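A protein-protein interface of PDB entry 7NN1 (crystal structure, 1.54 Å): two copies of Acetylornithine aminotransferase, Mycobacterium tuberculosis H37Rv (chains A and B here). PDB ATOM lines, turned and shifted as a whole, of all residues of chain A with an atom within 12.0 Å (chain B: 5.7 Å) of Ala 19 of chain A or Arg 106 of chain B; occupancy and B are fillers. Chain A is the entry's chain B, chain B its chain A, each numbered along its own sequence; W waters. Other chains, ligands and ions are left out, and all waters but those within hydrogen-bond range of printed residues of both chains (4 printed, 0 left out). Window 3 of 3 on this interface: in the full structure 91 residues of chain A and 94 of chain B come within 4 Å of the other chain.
Arg 108 of chain B touches Ala 19 of chain A. Thr 107 of chain B touches Val 20 of chain A (O to O, 3.9 Å). O of Val 20 of chain A touches CA of Arg 108 of chain B, at 3.1 Å. CE of Met 22 of chain A touches O of Arg 108 of chain B, at 3.5 Å. Met 22 of chain A touches Ala 268 of chain B.
N of Arg 108 of chain B sits at hydrogen-bond distance from O of Ala 268 of chain B. The backbone carbonyl oxygen of Met 22 of chain A lies close to the side-chain amide oxygen of Asn 24 of chain A (3.5 Å). OG1 of Thr 107 of chain B sits at hydrogen-bond distance from O of Gln 105 of chain B (3.4 Å). NE2 of Gln 18 of chain A sits at hydrogen-bond distance from OG1 of Thr 27 of chain A (3.2 Å). NE of Arg 108 of chain B lies within salt-bridge range of OE2 of Glu 274 of chain B, 3.1 Å away. O of Arg 106 of chain B is in hydrogen-bond range of N of Gly 270 of chain B, 2.8 Å away.
No position is printed for both chains. Of the 8 pairs that touch across the chains among the printed residues, none has its exchanged pair printed and touching as well.
Met 13 of chain A touches none of the printed residues of chain B. Of the printed residues of chain B, Gln 18 of chain A touches Arg 108 (2.7 Å). Of chain B, only Arg 106 and Arg 108 come within 4 Å of Ala 19 of chain A. Printed residues of chain B within 4 Å of Val 20 of chain A: Thr 107 and Arg 108. Of the printed residues of chain B, Met 21 of chain A touches Arg 108. Printed residues of chain B within 4 Å of Met 22 of chain A: Arg 108 and Ala 268. Asn 24 of chain A touches none of the printed residues of chain B. No residue of chain A comes within 4 Å of Gln 105 of chain B. Arg 108 of chain B touches just these residues of chain A: Gln 18, Ala 19, Val 20, Met 21 and Met 22. Ala 268 of chain B touches one residue of chain A. Val 269 of chain B touches none of the printed residues of chain A. No residue of chain A comes within 4 Å of Gly 270 of chain B. The nearest residue of chain B that does not touch Ala 19 of chain A is Thr 107 of chain B (4.4 Å).
NH1 of Arg 106 of chain B sits at hydrogen-bond distance from O of Ala 19 of chain A (2.9 Å). NH1 of Arg 108 of chain B sits at hydrogen-bond distance from O of Gln 18 of chain A (2.7 Å). The guanidinium group of Arg 108 of chain B lies within hydrogen-bond range of the backbone carbonyl oxygen of Met 21 of chain A (3.0 Å).
Hydrophobic or aromatic side chains of chain B within 4 Å of the printed part of chain A: Ala 268. Hydrophobic or aromatic side chains of chain A that line the printed part of chain B: Met 22. Among the printed residues, no Asp or Glu carboxylate lies within 4 Å of a Lys or Arg side-chain nitrogen of the other chain.
Water W3 lies within hydrogen-bond range of the backbone carbonyl oxygen of Thr 107 of chain B (2.7 Å) and the backbone carbonyl oxygen of Ala 19 of chain A (2.9 Å). Water W1 lies within hydrogen-bond range of O of Ala 273 of chain B and N of Asn 23 of chain A. Water W2 bridges the backbone carbonyl oxygen of Met 21 of chain A and the guanidinium group of Arg 108 of chain B. Water W4 bridges the backbone carbonyl oxygen (O) of Ala 273 of chain B (3.4 Å) and the side-chain sulfur (SD) of Met 22 of chain A (3.5 Å).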
ATOM      1  N   THR A  10       5.766 -13.265  -0.713  1.00  0.00           N
ATOM      2  CA  THR A  10       4.322 -13.086  -0.595  1.00  0.00           C
ATOM      3  C   THR A  10       3.987 -12.001   0.422  1.00  0.00           C
ATOM      4  O   THR A  10       3.055 -11.213   0.214  1.00  0.00           O
ATOM      5  CB  THR A  10       3.667 -14.419  -0.209  1.00  0.00           C
ATOM      6  OG1 THR A  10       3.774 -15.341  -1.305  1.00  0.00           O
ATOM      7  CG2 THR A  10       2.208 -14.225   0.148  1.00  0.00           C
ATOM      8  N   ALA A  11       4.754 -11.930   1.514  1.00  0.00           N
ATOM      9  CA  ALA A  11       4.523 -10.915   2.537  1.00  0.00           C
ATOM     10  C   ALA A  11       4.676  -9.504   1.978  1.00  0.00           C
ATOM     11  O   ALA A  11       3.865  -8.620   2.277  1.00  0.00           O
ATOM     12  CB  ALA A  11       5.485 -11.130   3.704  1.00  0.00           C
ATOM     13  N   THR A  12       5.717  -9.267   1.179  1.00  0.00           N
ATOM     14  CA  THR A  12       5.951  -7.927   0.649  1.00  0.00           C
ATOM     15  C   THR A  12       4.872  -7.540  -0.351  1.00  0.00           C
ATOM     16  O   THR A  12       4.415  -6.390  -0.369  1.00  0.00           O
ATOM     17  CB  THR A  12       7.328  -7.846  -0.003  1.00  0.00           C
ATOM     18  OG1 THR A  12       8.334  -8.101   0.983  1.00  0.00           O
ATOM     19  CG2 THR A  12       7.558  -6.465  -0.587  1.00  0.00           C
ATOM     20  N   MET A  13       4.451  -8.486  -1.190  1.00  0.00           N
ATOM     21  CA  MET A  13       3.410  -8.183  -2.167  1.00  0.00           C
ATOM     22  C   MET A  13       2.086  -7.865  -1.487  1.00  0.00           C
ATOM     23  O   MET A  13       1.357  -6.967  -1.927  1.00  0.00           O
ATOM     24  CB  MET A  13       3.254  -9.349  -3.140  1.00  0.00           C
ATOM     25  CG  MET A  13       4.322  -9.369  -4.190  1.00  0.00           C
ATOM     26  SD  MET A  13       3.896  -8.214  -5.498  1.00  0.00           S
ATOM     27  CE  MET A  13       2.588  -9.184  -6.264  1.00  0.00           C
ATOM     28  N   ARG A  14       1.758  -8.586  -0.411  1.00  0.00           N
ATOM     29  CA  ARG A  14       0.524  -8.305   0.314  1.00  0.00           C
ATOM     30  C   ARG A  14       0.606  -6.971   1.047  1.00  0.00           C
ATOM     31  O   ARG A  14      -0.394  -6.248   1.145  1.00  0.00           O
ATOM     32  CB  ARG A  14       0.197  -9.445   1.285  1.00  0.00           C
ATOM     33  CG  ARG A  14      -0.149 -10.764   0.587  1.00  0.00           C
ATOM     34  CD  ARG A  14      -0.407 -11.916   1.568  1.00  0.00           C
ATOM     35  NE  ARG A  14      -1.733 -11.856   2.178  1.00  0.00           N
ATOM     36  CZ  ARG A  14      -1.991 -11.301   3.358  1.00  0.00           C
ATOM     37  NH1 ARG A  14      -1.009 -10.757   4.066  1.00  0.00           N
ATOM     38  NH2 ARG A  14      -3.228 -11.286   3.832  1.00  0.00           N
ATOM     39  N   GLN A  15       1.781  -6.625   1.572  1.00  0.00           N
ATOM     40  CA  GLN A  15       1.930  -5.311   2.192  1.00  0.00           C
ATOM     41  C   GLN A  15       1.773  -4.206   1.156  1.00  0.00           C
ATOM     42  O   GLN A  15       1.137  -3.181   1.426  1.00  0.00           O
ATOM     43  CB  GLN A  15       3.278  -5.202   2.908  1.00  0.00           C
ATOM     44  CG  GLN A  15       3.366  -6.081   4.154  1.00  0.00           C
ATOM     45  CD  GLN A  15       4.790  -6.477   4.512  1.00  0.00           C
ATOM     46  OE1 GLN A  15       5.749  -6.079   3.842  1.00  0.00           O
ATOM     47  NE2 GLN A  15       4.933  -7.268   5.573  1.00  0.00           N
ATOM     48  N   ARG A  16       2.324  -4.406  -0.044  1.00  0.00           N
ATOM     49  CA  ARG A  16       2.148  -3.405  -1.095  1.00  0.00           C
ATOM     50  C   ARG A  16       0.682  -3.288  -1.487  1.00  0.00           C
ATOM     51  O   ARG A  16       0.168  -2.179  -1.681  1.00  0.00           O
ATOM     52  CB  ARG A  16       3.003  -3.742  -2.314  1.00  0.00           C
ATOM     53  CG  ARG A  16       4.501  -3.595  -2.100  1.00  0.00           C
ATOM     54  CD  ARG A  16       5.257  -4.133  -3.298  1.00  0.00           C
ATOM     55  NE  ARG A  16       4.955  -3.377  -4.510  1.00  0.00           N
ATOM     56  CZ  ARG A  16       5.214  -3.810  -5.736  1.00  0.00           C
ATOM     57  NH1 ARG A  16       5.772  -5.000  -5.915  1.00  0.00           N
ATOM     58  NH2 ARG A  16       4.913  -3.058  -6.790  1.00  0.00           N
ATOM     59  N   TRP A  17      -0.010  -4.424  -1.600  1.00  0.00           N
ATOM     60  CA  TRP A  17      -1.447  -4.400  -1.858  1.00  0.00           C
ATOM     61  C   TRP A  17      -2.176  -3.577  -0.807  1.00  0.00           C
ATOM     62  O   TRP A  17      -2.935  -2.655  -1.137  1.00  0.00           O
ATOM     63  CB  TRP A  17      -1.993  -5.834  -1.899  1.00  0.00           C
ATOM     64  CG  TRP A  17      -3.482  -5.922  -2.017  1.00  0.00           C
ATOM     65  CD1 TRP A  17      -4.403  -5.720  -1.028  1.00  0.00           C
ATOM     66  CD2 TRP A  17      -4.232  -6.252  -3.198  1.00  0.00           C
ATOM     67  NE1 TRP A  17      -5.670  -5.889  -1.520  1.00  0.00           N
ATOM     68  CE2 TRP A  17      -5.593  -6.227  -2.844  1.00  0.00           C
ATOM     69  CE3 TRP A  17      -3.879  -6.577  -4.509  1.00  0.00           C
ATOM     70  CZ2 TRP A  17      -6.610  -6.501  -3.760  1.00  0.00           C
ATOM     71  CZ3 TRP A  17      -4.886  -6.846  -5.425  1.00  0.00           C
ATOM     72  CH2 TRP A  17      -6.234  -6.806  -5.043  1.00  0.00           C
ATOM     73  N   GLN A  18      -1.956  -3.889   0.471  1.00  0.00           N
ATOM     74  CA  GLN A  18      -2.707  -3.218   1.526  1.00  0.00           C
ATOM     75  C   GLN A  18      -2.395  -1.732   1.620  1.00  0.00           C
ATOM     76  O   GLN A  18      -3.192  -0.986   2.201  1.00  0.00           O
ATOM     77  CB  GLN A  18      -2.441  -3.881   2.882  1.00  0.00           C
ATOM     78  CG  GLN A  18      -3.125  -5.215   3.055  1.00  0.00           C
ATOM     79  CD  GLN A  18      -2.529  -6.034   4.191  1.00  0.00           C
ATOM     80  OE1 GLN A  18      -1.347  -5.907   4.516  1.00  0.00           O
ATOM     81  NE2 GLN A  18      -3.349  -6.880   4.797  1.00  0.00           N
ATOM     82  N   ALA A  19      -1.263  -1.286   1.073  1.00  0.00           N
ATOM     83  CA  ALA A  19      -0.921   0.132   1.131  1.00  0.00           C
ATOM     84  C   ALA A  19      -1.637   0.962   0.070  1.00  0.00           C
ATOM     85  O   ALA A  19      -1.755   2.183   0.246  1.00  0.00           O
ATOM     86  CB  ALA A  19       0.592   0.327   0.991  1.00  0.00           C
ATOM     87  N   VAL A  20      -2.114   0.347  -1.017  1.00  0.00           N
ATOM     88  CA  VAL A  20      -2.577   1.142  -2.159  1.00  0.00           C
ATOM     89  C   VAL A  20      -3.939   0.700  -2.692  1.00  0.00           C
ATOM     90  O   VAL A  20      -4.679   1.515  -3.262  1.00  0.00           O
ATOM     91  CB  VAL A  20      -1.527   1.131  -3.290  1.00  0.00           C
ATOM     92  CG1 VAL A  20      -1.476  -0.220  -4.014  1.00  0.00           C
ATOM     93  CG2 VAL A  20      -1.777   2.265  -4.279  1.00  0.00           C
ATOM     94  N   MET A  21      -4.296  -0.576  -2.529  1.00  0.00           N
ATOM     95  CA  MET A  21      -5.551  -1.023  -3.117  1.00  0.00           C
ATOM     96  C   MET A  21      -6.721  -0.684  -2.205  1.00  0.00           C
ATOM     97  O   MET A  21      -6.604  -0.704  -0.980  1.00  0.00           O
ATOM     98  CB  MET A  21      -5.531  -2.542  -3.382  1.00  0.00           C
ATOM     99  CG  MET A  21      -4.447  -3.015  -4.346  1.00  0.00           C
ATOM    100  SD  MET A  21      -4.392  -2.129  -5.918  1.00  0.00           S
ATOM    101  CE  MET A  21      -6.071  -2.376  -6.521  1.00  0.00           C
ATOM    102  N   MET A  22      -7.877  -0.384  -2.806  1.00  0.00           N
ATOM    103  CA  MET A  22      -9.074  -0.351  -1.985  1.00  0.00           C
ATOM    104  C   MET A  22      -9.336  -1.743  -1.425  1.00  0.00           C
ATOM    105  O   MET A  22      -8.939  -2.751  -2.007  1.00  0.00           O
ATOM    106  CB  MET A  22     -10.274   0.133  -2.781  1.00  0.00           C
ATOM    107  CG  MET A  22     -10.312   1.641  -2.855  1.00  0.00           C
ATOM    108  SD  MET A  22     -11.823   2.153  -3.624  1.00  0.00           S
ATOM    109  CE  MET A  22     -11.237   3.501  -4.654  1.00  0.00           C
ATOM    110  N   ASN A  23     -10.007  -1.787  -0.279  1.00  0.00           N
ATOM    111  CA  ASN A  23     -10.232  -3.034   0.441  1.00  0.00           C
ATOM    112  C   ASN A  23     -11.545  -3.716   0.053  1.00  0.00           C
ATOM    113  O   ASN A  23     -12.143  -4.421   0.880  1.00  0.00           O
ATOM    114  CB  ASN A  23     -10.176  -2.769   1.949  1.00  0.00           C
ATOM    115  CG  ASN A  23      -9.955  -4.040   2.765  1.00  0.00           C
ATOM    116  OD1 ASN A  23      -9.315  -4.988   2.303  1.00  0.00           O
ATOM    117  ND2 ASN A  23     -10.491  -4.061   3.981  1.00  0.00           N
ATOM    118  N   ASN A  24     -12.012  -3.545  -1.189  1.00  0.00           N
ATOM    119  CA  ASN A  24     -13.278  -4.167  -1.578  1.00  0.00           C
ATOM    120  C   ASN A  24     -13.163  -5.677  -1.801  1.00  0.00           C
ATOM    121  O   ASN A  24     -14.194  -6.351  -1.866  1.00  0.00           O
ATOM    122  CB  ASN A  24     -13.823  -3.496  -2.844  1.00  0.00           C
ATOM    123  CG  ASN A  24     -12.852  -3.590  -3.998  1.00  0.00           C
ATOM    124  OD1 ASN A  24     -11.795  -2.951  -3.991  1.00  0.00           O
ATOM    125  ND2 ASN A  24     -13.181  -4.415  -4.981  1.00  0.00           N
ATOM    126  N   GLY A  26     -10.811  -7.497   0.206  1.00  0.00           N
ATOM    127  CA  GLY A  26      -9.913  -8.022   1.210  1.00  0.00           C
ATOM    128  C   GLY A  26      -8.512  -8.084   0.624  1.00  0.00           C
ATOM    129  O   GLY A  26      -8.221  -7.523  -0.438  1.00  0.00           O
ATOM    130  N   THR A  27      -7.631  -8.789   1.335  1.00  0.00           N
ATOM    131  CA  THR A  27      -6.251  -8.929   0.892  1.00  0.00           C
ATOM    132  C   THR A  27      -6.038 -10.337   0.363  1.00  0.00           C
ATOM    133  O   THR A  27      -6.255 -11.301   1.112  1.00  0.00           O
ATOM    134  CB  THR A  27      -5.277  -8.636   2.031  1.00  0.00           C
ATOM    135  OG1 THR A  27      -5.557  -7.340   2.575  1.00  0.00           O
ATOM    136  CG2 THR A  27      -3.851  -8.688   1.532  1.00  0.00           C
ATOM    137  N   PRO A  28      -5.647 -10.505  -0.899  1.00  0.00           N
ATOM    138  CA  PRO A  28      -5.453 -11.855  -1.450  1.00  0.00           C
ATOM    139  C   PRO A  28      -4.477 -12.659  -0.612  1.00  0.00           C
ATOM    140  O   PRO A  28      -3.421 -12.149  -0.209  1.00  0.00           O
ATOM    141  CB  PRO A  28      -4.885 -11.593  -2.850  1.00  0.00           C
ATOM    142  CG  PRO A  28      -5.418 -10.225  -3.229  1.00  0.00           C
ATOM    143  CD  PRO A  28      -5.578  -9.452  -1.935  1.00  0.00           C
ATOM    144  N   ASP B 104      -2.396  14.693  -0.464  1.00  0.00           N
ATOM    145  CA  ASP B 104      -1.768  14.766   0.852  1.00  0.00           C
ATOM    146  C   ASP B 104      -2.116  13.548   1.705  1.00  0.00           C
ATOM    147  O   ASP B 104      -1.283  13.068   2.482  1.00  0.00           O
ATOM    148  CB  ASP B 104      -2.190  16.054   1.559  1.00  0.00           C
ATOM    149  CG  ASP B 104      -3.706  16.215   1.634  1.00  0.00           C
ATOM    150  OD1 ASP B 104      -4.427  15.548   0.854  1.00  0.00           O
ATOM    151  OD2 ASP B 104      -4.179  17.005   2.483  1.00  0.00           O
ATOM    152  N   GLN B 105      -3.329  13.029   1.572  1.00  0.00           N
ATOM    153  CA  GLN B 105      -3.781  11.908   2.383  1.00  0.00           C
ATOM    154  C   GLN B 105      -3.626  10.597   1.625  1.00  0.00           C
ATOM    155  O   GLN B 105      -3.306  10.569   0.435  1.00  0.00           O
ATOM    156  CB  GLN B 105      -5.236  12.096   2.808  1.00  0.00           C
ATOM    157  CG  GLN B 105      -5.501  13.378   3.555  1.00  0.00           C
ATOM    158  CD  GLN B 105      -6.878  13.918   3.272  1.00  0.00           C
ATOM    159  OE1 GLN B 105      -7.088  14.635   2.293  1.00  0.00           O
ATOM    160  NE2 GLN B 105      -7.833  13.570   4.122  1.00  0.00           N
ATOM    161  N   ARG B 106      -3.861   9.496   2.337  1.00  0.00           N
ATOM    162  CA  ARG B 106      -3.766   8.190   1.701  1.00  0.00           C
ATOM    163  C   ARG B 106      -4.786   8.082   0.577  1.00  0.00           C
ATOM    164  O   ARG B 106      -5.935   8.505   0.716  1.00  0.00           O
ATOM    165  CB  ARG B 106      -3.990   7.062   2.709  1.00  0.00           C
ATOM    166  CG  ARG B 106      -3.948   5.683   2.039  1.00  0.00           C
ATOM    167  CD  ARG B 106      -3.869   4.552   3.026  1.00  0.00           C
ATOM    168  NE  ARG B 106      -2.775   4.721   3.973  1.00  0.00           N
ATOM    169  CZ  ARG B 106      -1.522   4.337   3.753  1.00  0.00           C
ATOM    170  NH1 ARG B 106      -1.182   3.754   2.606  1.00  0.00           N
ATOM    171  NH2 ARG B 106      -0.604   4.533   4.689  1.00  0.00           N
ATOM    172  N   THR B 107      -4.344   7.520  -0.541  1.00  0.00           N
ATOM    173  CA  THR B 107      -5.155   7.304  -1.726  1.00  0.00           C
ATOM    174  C   THR B 107      -5.204   5.811  -2.011  1.00  0.00           C
ATOM    175  O   THR B 107      -4.173   5.134  -1.947  1.00  0.00           O
ATOM    176  CB  THR B 107      -4.555   8.034  -2.925  1.00  0.00           C
ATOM    177  OG1 THR B 107      -4.325   9.400  -2.562  1.00  0.00           O
ATOM    178  CG2 THR B 107      -5.495   7.959  -4.124  1.00  0.00           C
ATOM    179  N   ARG B 108      -6.396   5.301  -2.327  1.00  0.00           N
ATOM    180  CA  ARG B 108      -6.563   3.898  -2.678  1.00  0.00           C
ATOM    181  C   ARG B 108      -7.216   3.768  -4.049  1.00  0.00           C
ATOM    182  O   ARG B 108      -7.943   4.663  -4.498  1.00  0.00           O
ATOM    183  CB  ARG B 108      -7.377   3.156  -1.614  1.00  0.00           C
ATOM    184  CG  ARG B 108      -6.639   3.075  -0.290  1.00  0.00           C
ATOM    185  CD  ARG B 108      -7.382   2.234   0.740  1.00  0.00           C
ATOM    186  NE  ARG B 108      -6.648   2.206   1.999  1.00  0.00           N
ATOM    187  CZ  ARG B 108      -5.587   1.438   2.222  1.00  0.00           C
ATOM    188  NH1 ARG B 108      -5.145   0.613   1.273  1.00  0.00           N
ATOM    189  NH2 ARG B 108      -4.970   1.485   3.397  1.00  0.00           N
ATOM    190  N   ALA B 268      -9.602   7.104  -4.791  1.00  0.00           N
ATOM    191  CA  ALA B 268     -10.297   7.769  -3.695  1.00  0.00           C
ATOM    192  C   ALA B 268      -9.289   8.213  -2.644  1.00  0.00           C
ATOM    193  O   ALA B 268      -8.353   7.476  -2.322  1.00  0.00           O
ATOM    194  CB  ALA B 268     -11.358   6.861  -3.062  1.00  0.00           C
ATOM    195  N   VAL B 269      -9.513   9.398  -2.078  1.00  0.00           N
ATOM    196  CA  VAL B 269      -8.529  10.092  -1.254  1.00  0.00           C
ATOM    197  C   VAL B 269      -9.100  10.264   0.145  1.00  0.00           C
ATOM    198  O   VAL B 269     -10.257  10.660   0.300  1.00  0.00           O
ATOM    199  CB  VAL B 269      -8.160  11.462  -1.859  1.00  0.00           C
ATOM    200  CG1 VAL B 269      -7.225  12.231  -0.926  1.00  0.00           C
ATOM    201  CG2 VAL B 269      -7.529  11.277  -3.225  1.00  0.00           C
ATOM    202  N   GLY B 270      -8.292   9.959   1.160  1.00  0.00           N
ATOM    203  CA  GLY B 270      -8.676  10.203   2.530  1.00  0.00           C
ATOM    204  C   GLY B 270      -9.788   9.285   2.999  1.00  0.00           C
ATOM    205  O   GLY B 270      -9.796   8.086   2.701  1.00  0.00           O
ATOM    206  N   ALA B 273     -11.330   6.782   0.714  1.00  0.00           N
ATOM    207  CA  ALA B 273     -10.571   5.598   0.332  1.00  0.00           C
ATOM    208  C   ALA B 273     -10.897   4.391   1.207  1.00  0.00           C
ATOM    209  O   ALA B 273     -10.609   3.255   0.813  1.00  0.00           O
ATOM    210  CB  ALA B 273      -9.073   5.896   0.391  1.00  0.00           C
ATOM    211  N   GLU B 274     -11.499   4.609   2.367  1.00  0.00           N
ATOM    212  CA  GLU B 274     -11.804   3.544   3.315  1.00  0.00           C
ATOM    213  C   GLU B 274     -13.256   3.099   3.264  1.00  0.00           C
ATOM    214  O   GLU B 274     -13.640   2.200   4.018  1.00  0.00           O
ATOM    215  CB  GLU B 274     -11.456   3.998   4.734  1.00  0.00           C
ATOM    216  CG  GLU B 274     -10.105   4.695   4.826  1.00  0.00           C
ATOM    217  CD  GLU B 274      -8.947   3.802   4.416  1.00  0.00           C
ATOM    218  OE1 GLU B 274      -8.975   2.591   4.734  1.00  0.00           O
ATOM    219  OE2 GLU B 274      -7.999   4.313   3.779  1.00  0.00           O
HETATM  220  O   HOH W   1     -11.348   0.667   0.632  1.00  0.00           O
HETATM  221  O   HOH W   2      -6.028  -2.733   0.993  1.00  0.00           O
HETATM  222  O   HOH W   3      -1.613   4.539  -1.362  1.00  0.00           O
HETATM  223  O   HOH W   4     -13.574   3.144  -0.743  1.00  0.00           O
